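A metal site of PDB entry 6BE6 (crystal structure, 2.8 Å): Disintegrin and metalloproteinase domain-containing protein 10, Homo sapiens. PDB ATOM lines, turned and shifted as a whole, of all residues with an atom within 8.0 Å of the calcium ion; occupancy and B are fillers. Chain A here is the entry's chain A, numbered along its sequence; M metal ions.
The side-chain carboxylate (OE2) of Glu 256 sits close to the backbone NH (N) of Glu 253.
The side-chain amide oxygen of Asn 249 sits close to the backbone carbonyl oxygen of Met 251 (3.2 Å).
ND2 of Asn 249 sits at hydrogen-bond distance from OE2 of Glu 253 (2.4 Å).
The side-chain amide nitrogen of Asn 249 sits at hydrogen-bond distance from the backbone carbonyl oxygen of Val 59.
The backbone NH (N) of Gly 248 lies within hydrogen-bond range of the side-chain carboxylate (OD1) of Asp 259 (3.3 Å).
The side-chain carboxylate (OD1) of Asp 259 lies within hydrogen-bond range of the backbone NH (N) of Gly 250 (2.9 Å).
SG of Cys 282 is disulfide-bonded to SG of Cys 247.
The calcium ion is bound by the side-chain carboxylate of Glu 256 (2.3 Å), the side-chain amide oxygen of Asn 249 (2.4 Å), the side-chain carboxylate of Asp 259 (2.4 Å) and the backbone carbonyl oxygen of Ile 246 (2.5 Å).
The calcium ion has four donor atoms within binding distance.
Slightly farther from the calcium ion lies OE1 of Glu 256 (3.0 Å).
Slightly farther from the calcium ion lies O of Met 251 (3.0 Å).
Merely in contact with the calcium ion: Glu 253.
Six residues have an atom within 4 Å of the calcium ion: Ile 246, Asn 249, Met 251, Glu 253, Glu 256 and Asp 259.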
ATOM      1  N   MET A  58       9.195 -13.961 -24.727  1.00  0.00           N
ATOM      2  CA  MET A  58      10.642 -13.866 -24.629  1.00  0.00           C
ATOM      3  C   MET A  58      11.057 -14.273 -23.217  1.00  0.00           C
ATOM      4  O   MET A  58      10.364 -13.953 -22.248  1.00  0.00           O
ATOM      5  CB  MET A  58      11.140 -12.461 -24.956  1.00  0.00           C
ATOM      6  CG  MET A  58      12.653 -12.350 -25.052  1.00  0.00           C
ATOM      7  SD  MET A  58      13.178 -11.315 -26.422  1.00  0.00           S
ATOM      8  CE  MET A  58      12.392 -12.166 -27.791  1.00  0.00           C
ATOM      9  N   VAL A  59      12.178 -14.983 -23.118  1.00  0.00           N
ATOM     10  CA  VAL A  59      12.699 -15.435 -21.836  1.00  0.00           C
ATOM     11  C   VAL A  59      13.607 -14.352 -21.264  1.00  0.00           C
ATOM     12  O   VAL A  59      14.613 -13.991 -21.885  1.00  0.00           O
ATOM     13  CB  VAL A  59      13.449 -16.762 -21.971  1.00  0.00           C
ATOM     14  CG1 VAL A  59      14.020 -17.177 -20.623  1.00  0.00           C
ATOM     15  CG2 VAL A  59      12.538 -17.838 -22.527  1.00  0.00           C
ATOM     16  N   LYS A  60      13.262 -13.844 -20.088  1.00  0.00           N
ATOM     17  CA  LYS A  60      14.078 -12.824 -19.441  1.00  0.00           C
ATOM     18  C   LYS A  60      15.095 -13.412 -18.470  1.00  0.00           C
ATOM     19  O   LYS A  60      16.136 -12.790 -18.227  1.00  0.00           O
ATOM     20  CB  LYS A  60      13.191 -11.823 -18.696  1.00  0.00           C
ATOM     21  CG  LYS A  60      13.898 -10.543 -18.292  1.00  0.00           C
ATOM     22  CD  LYS A  60      12.944  -9.571 -17.607  1.00  0.00           C
ATOM     23  CE  LYS A  60      13.663  -8.277 -17.219  1.00  0.00           C
ATOM     24  NZ  LYS A  60      12.744  -7.314 -16.554  1.00  0.00           N
ATOM     25  N   GLN A 244      16.039  -6.102 -29.225  1.00  0.00           N
ATOM     26  CA  GLN A 244      17.069  -7.121 -29.333  1.00  0.00           C
ATOM     27  C   GLN A 244      17.016  -8.049 -28.123  1.00  0.00           C
ATOM     28  O   GLN A 244      16.532  -7.670 -27.052  1.00  0.00           O
ATOM     29  CB  GLN A 244      18.450  -6.465 -29.437  1.00  0.00           C
ATOM     30  CG  GLN A 244      18.843  -5.660 -28.218  1.00  0.00           C
ATOM     31  CD  GLN A 244      20.212  -5.022 -28.368  1.00  0.00           C
ATOM     32  OE1 GLN A 244      20.769  -4.974 -29.465  1.00  0.00           O
ATOM     33  NE2 GLN A 244      20.764  -4.529 -27.260  1.00  0.00           N
ATOM     34  N   PRO A 245      17.505  -9.286 -28.264  1.00  0.00           N
ATOM     35  CA  PRO A 245      17.522 -10.205 -27.125  1.00  0.00           C
ATOM     36  C   PRO A 245      18.411  -9.685 -26.003  1.00  0.00           C
ATOM     37  O   PRO A 245      19.441  -9.044 -26.242  1.00  0.00           O
ATOM     38  CB  PRO A 245      18.071 -11.500 -27.718  1.00  0.00           C
ATOM     39  CG  PRO A 245      17.792 -11.401 -29.178  1.00  0.00           C
ATOM     40  CD  PRO A 245      17.930  -9.951 -29.508  1.00  0.00           C
ATOM     41  N   ILE A 246      18.007  -9.952 -24.782  1.00  0.00           N
ATOM     42  CA  ILE A 246      18.716  -9.465 -23.607  1.00  0.00           C
ATOM     43  C   ILE A 246      19.843 -10.433 -23.268  1.00  0.00           C
ATOM     44  O   ILE A 246      19.759 -11.644 -23.513  1.00  0.00           O
ATOM     45  CB  ILE A 246      17.768  -9.284 -22.410  1.00  0.00           C
ATOM     46  CG1 ILE A 246      17.247 -10.637 -21.919  1.00  0.00           C
ATOM     47  CG2 ILE A 246      16.607  -8.370 -22.780  1.00  0.00           C
ATOM     48  CD1 ILE A 246      16.658 -10.590 -20.538  1.00  0.00           C
ATOM     49  N   CYS A 247      20.904  -9.891 -22.699  1.00  0.00           N
ATOM     50  CA  CYS A 247      22.043 -10.674 -22.258  1.00  0.00           C
ATOM     51  C   CYS A 247      21.832 -11.101 -20.809  1.00  0.00           C
ATOM     52  O   CYS A 247      21.492 -10.266 -19.962  1.00  0.00           O
ATOM     53  CB  CYS A 247      23.345  -9.886 -22.392  1.00  0.00           C
ATOM     54  SG  CYS A 247      24.741 -10.604 -21.519  1.00  0.00           S
ATOM     55  N   GLY A 248      22.017 -12.394 -20.537  1.00  0.00           N
ATOM     56  CA  GLY A 248      21.870 -12.930 -19.196  1.00  0.00           C
ATOM     57  C   GLY A 248      20.681 -13.832 -18.989  1.00  0.00           C
ATOM     58  O   GLY A 248      20.463 -14.283 -17.860  1.00  0.00           O
ATOM     59  N   ASN A 249      19.914 -14.134 -20.033  1.00  0.00           N
ATOM     60  CA  ASN A 249      18.778 -15.039 -19.901  1.00  0.00           C
ATOM     61  C   ASN A 249      19.178 -16.507 -19.977  1.00  0.00           C
ATOM     62  O   ASN A 249      18.301 -17.373 -19.972  1.00  0.00           O
ATOM     63  CB  ASN A 249      17.722 -14.726 -20.968  1.00  0.00           C
ATOM     64  CG  ASN A 249      18.215 -14.975 -22.372  1.00  0.00           C
ATOM     65  OD1 ASN A 249      19.414 -14.950 -22.639  1.00  0.00           O
ATOM     66  ND2 ASN A 249      17.279 -15.218 -23.285  1.00  0.00           N
ATOM     67  N   GLY A 250      20.473 -16.808 -20.052  1.00  0.00           N
ATOM     68  CA  GLY A 250      20.947 -18.172 -20.047  1.00  0.00           C
ATOM     69  C   GLY A 250      20.829 -18.901 -21.358  1.00  0.00           C
ATOM     70  O   GLY A 250      21.158 -20.099 -21.415  1.00  0.00           O
ATOM     71  N   MET A 251      20.378 -18.247 -22.426  1.00  0.00           N
ATOM     72  CA  MET A 251      20.243 -18.866 -23.727  1.00  0.00           C
ATOM     73  C   MET A 251      20.992 -18.034 -24.756  1.00  0.00           C
ATOM     74  O   MET A 251      20.790 -16.818 -24.850  1.00  0.00           O
ATOM     75  CB  MET A 251      18.772 -19.012 -24.126  1.00  0.00           C
ATOM     76  CG  MET A 251      18.193 -20.386 -23.809  1.00  0.00           C
ATOM     77  SD  MET A 251      16.412 -20.475 -24.054  1.00  0.00           S
ATOM     78  CE  MET A 251      15.870 -19.394 -22.746  1.00  0.00           C
ATOM     79  N   VAL A 252      21.871 -18.691 -25.524  1.00  0.00           N
ATOM     80  CA  VAL A 252      22.609 -17.995 -26.577  1.00  0.00           C
ATOM     81  C   VAL A 252      21.673 -17.685 -27.725  1.00  0.00           C
ATOM     82  O   VAL A 252      20.991 -18.564 -28.261  1.00  0.00           O
ATOM     83  CB  VAL A 252      23.818 -18.827 -27.031  1.00  0.00           C
ATOM     84  CG1 VAL A 252      24.859 -18.890 -25.927  1.00  0.00           C
ATOM     85  CG2 VAL A 252      23.391 -20.233 -27.428  1.00  0.00           C
ATOM     86  N   GLU A 253      21.623 -16.411 -28.114  1.00  0.00           N
ATOM     87  CA  GLU A 253      20.746 -15.951 -29.175  1.00  0.00           C
ATOM     88  C   GLU A 253      21.564 -15.159 -30.187  1.00  0.00           C
ATOM     89  O   GLU A 253      22.792 -15.071 -30.087  1.00  0.00           O
ATOM     90  CB  GLU A 253      19.591 -15.115 -28.604  1.00  0.00           C
ATOM     91  CG  GLU A 253      18.865 -15.806 -27.455  1.00  0.00           C
ATOM     92  CD  GLU A 253      17.722 -14.985 -26.895  1.00  0.00           C
ATOM     93  OE1 GLU A 253      16.925 -14.455 -27.684  1.00  0.00           O
ATOM     94  OE2 GLU A 253      17.638 -14.874 -25.655  1.00  0.00           O
ATOM     95  N   GLN A 254      20.882 -14.605 -31.169  1.00  0.00           N
ATOM     96  CA  GLN A 254      21.564 -13.909 -32.253  1.00  0.00           C
ATOM     97  C   GLN A 254      22.162 -12.593 -31.748  1.00  0.00           C
ATOM     98  O   GLN A 254      21.465 -11.761 -31.169  1.00  0.00           O
ATOM     99  CB  GLN A 254      20.605 -13.647 -33.406  1.00  0.00           C
ATOM    100  CG  GLN A 254      21.254 -13.072 -34.633  1.00  0.00           C
ATOM    101  CD  GLN A 254      20.264 -12.920 -35.768  1.00  0.00           C
ATOM    102  OE1 GLN A 254      20.631 -12.510 -36.875  1.00  0.00           O
ATOM    103  NE2 GLN A 254      19.012 -13.253 -35.499  1.00  0.00           N
ATOM    104  N   GLY A 255      23.462 -12.417 -31.977  1.00  0.00           N
ATOM    105  CA  GLY A 255      24.161 -11.217 -31.563  1.00  0.00           C
ATOM    106  C   GLY A 255      25.044 -11.388 -30.348  1.00  0.00           C
ATOM    107  O   GLY A 255      25.706 -10.421 -29.945  1.00  0.00           O
ATOM    108  N   GLU A 256      25.079 -12.579 -29.743  1.00  0.00           N
ATOM    109  CA  GLU A 256      25.901 -12.854 -28.575  1.00  0.00           C
ATOM    110  C   GLU A 256      26.601 -14.193 -28.772  1.00  0.00           C
ATOM    111  O   GLU A 256      26.025 -15.123 -29.336  1.00  0.00           O
ATOM    112  CB  GLU A 256      25.048 -12.881 -27.302  1.00  0.00           C
ATOM    113  CG  GLU A 256      23.879 -13.839 -27.365  1.00  0.00           C
ATOM    114  CD  GLU A 256      22.914 -13.690 -26.208  1.00  0.00           C
ATOM    115  OE1 GLU A 256      23.154 -12.825 -25.341  1.00  0.00           O
ATOM    116  OE2 GLU A 256      21.912 -14.433 -26.188  1.00  0.00           O
ATOM    117  N   CYS A 258      28.157 -16.107 -26.200  1.00  0.00           N
ATOM    118  CA  CYS A 258      27.789 -16.998 -25.120  1.00  0.00           C
ATOM    119  C   CYS A 258      26.785 -16.289 -24.216  1.00  0.00           C
ATOM    120  O   CYS A 258      26.497 -15.107 -24.384  1.00  0.00           O
ATOM    121  CB  CYS A 258      29.027 -17.448 -24.316  1.00  0.00           C
ATOM    122  SG  CYS A 258      29.985 -16.090 -23.613  1.00  0.00           S
ATOM    123  N   ASP A 259      26.241 -17.039 -23.258  1.00  0.00           N
ATOM    124  CA  ASP A 259      25.205 -16.496 -22.372  1.00  0.00           C
ATOM    125  C   ASP A 259      25.080 -17.450 -21.173  1.00  0.00           C
ATOM    126  O   ASP A 259      24.336 -18.428 -21.234  1.00  0.00           O
ATOM    127  CB  ASP A 259      23.880 -16.336 -23.100  1.00  0.00           C
ATOM    128  CG  ASP A 259      22.900 -15.450 -22.348  1.00  0.00           C
ATOM    129  OD1 ASP A 259      22.816 -15.550 -21.108  1.00  0.00           O
ATOM    130  OD2 ASP A 259      22.216 -14.634 -23.004  1.00  0.00           O
ATOM    131  N   CYS A 260      25.794 -17.131 -20.102  1.00  0.00           N
ATOM    132  CA  CYS A 260      25.710 -17.929 -18.880  1.00  0.00           C
ATOM    133  C   CYS A 260      24.705 -17.370 -17.892  1.00  0.00           C
ATOM    134  O   CYS A 260      24.091 -18.142 -17.142  1.00  0.00           O
ATOM    135  CB  CYS A 260      27.086 -18.036 -18.206  1.00  0.00           C
ATOM    136  SG  CYS A 260      27.854 -16.452 -17.808  1.00  0.00           S
ATOM    137  N   CYS A 282      28.202 -11.217 -22.320  1.00  0.00           N
ATOM    138  CA  CYS A 282      27.711 -12.250 -23.236  1.00  0.00           C
ATOM    139  C   CYS A 282      28.651 -12.427 -24.431  1.00  0.00           C
ATOM    140  O   CYS A 282      28.216 -12.726 -25.546  1.00  0.00           O
ATOM    141  CB  CYS A 282      26.287 -11.956 -23.721  1.00  0.00           C
ATOM    142  SG  CYS A 282      25.037 -12.361 -22.495  1.00  0.00           S
HETATM  143 CA    CA M   1      20.466 -13.824 -24.452  1.00  0.00          CA
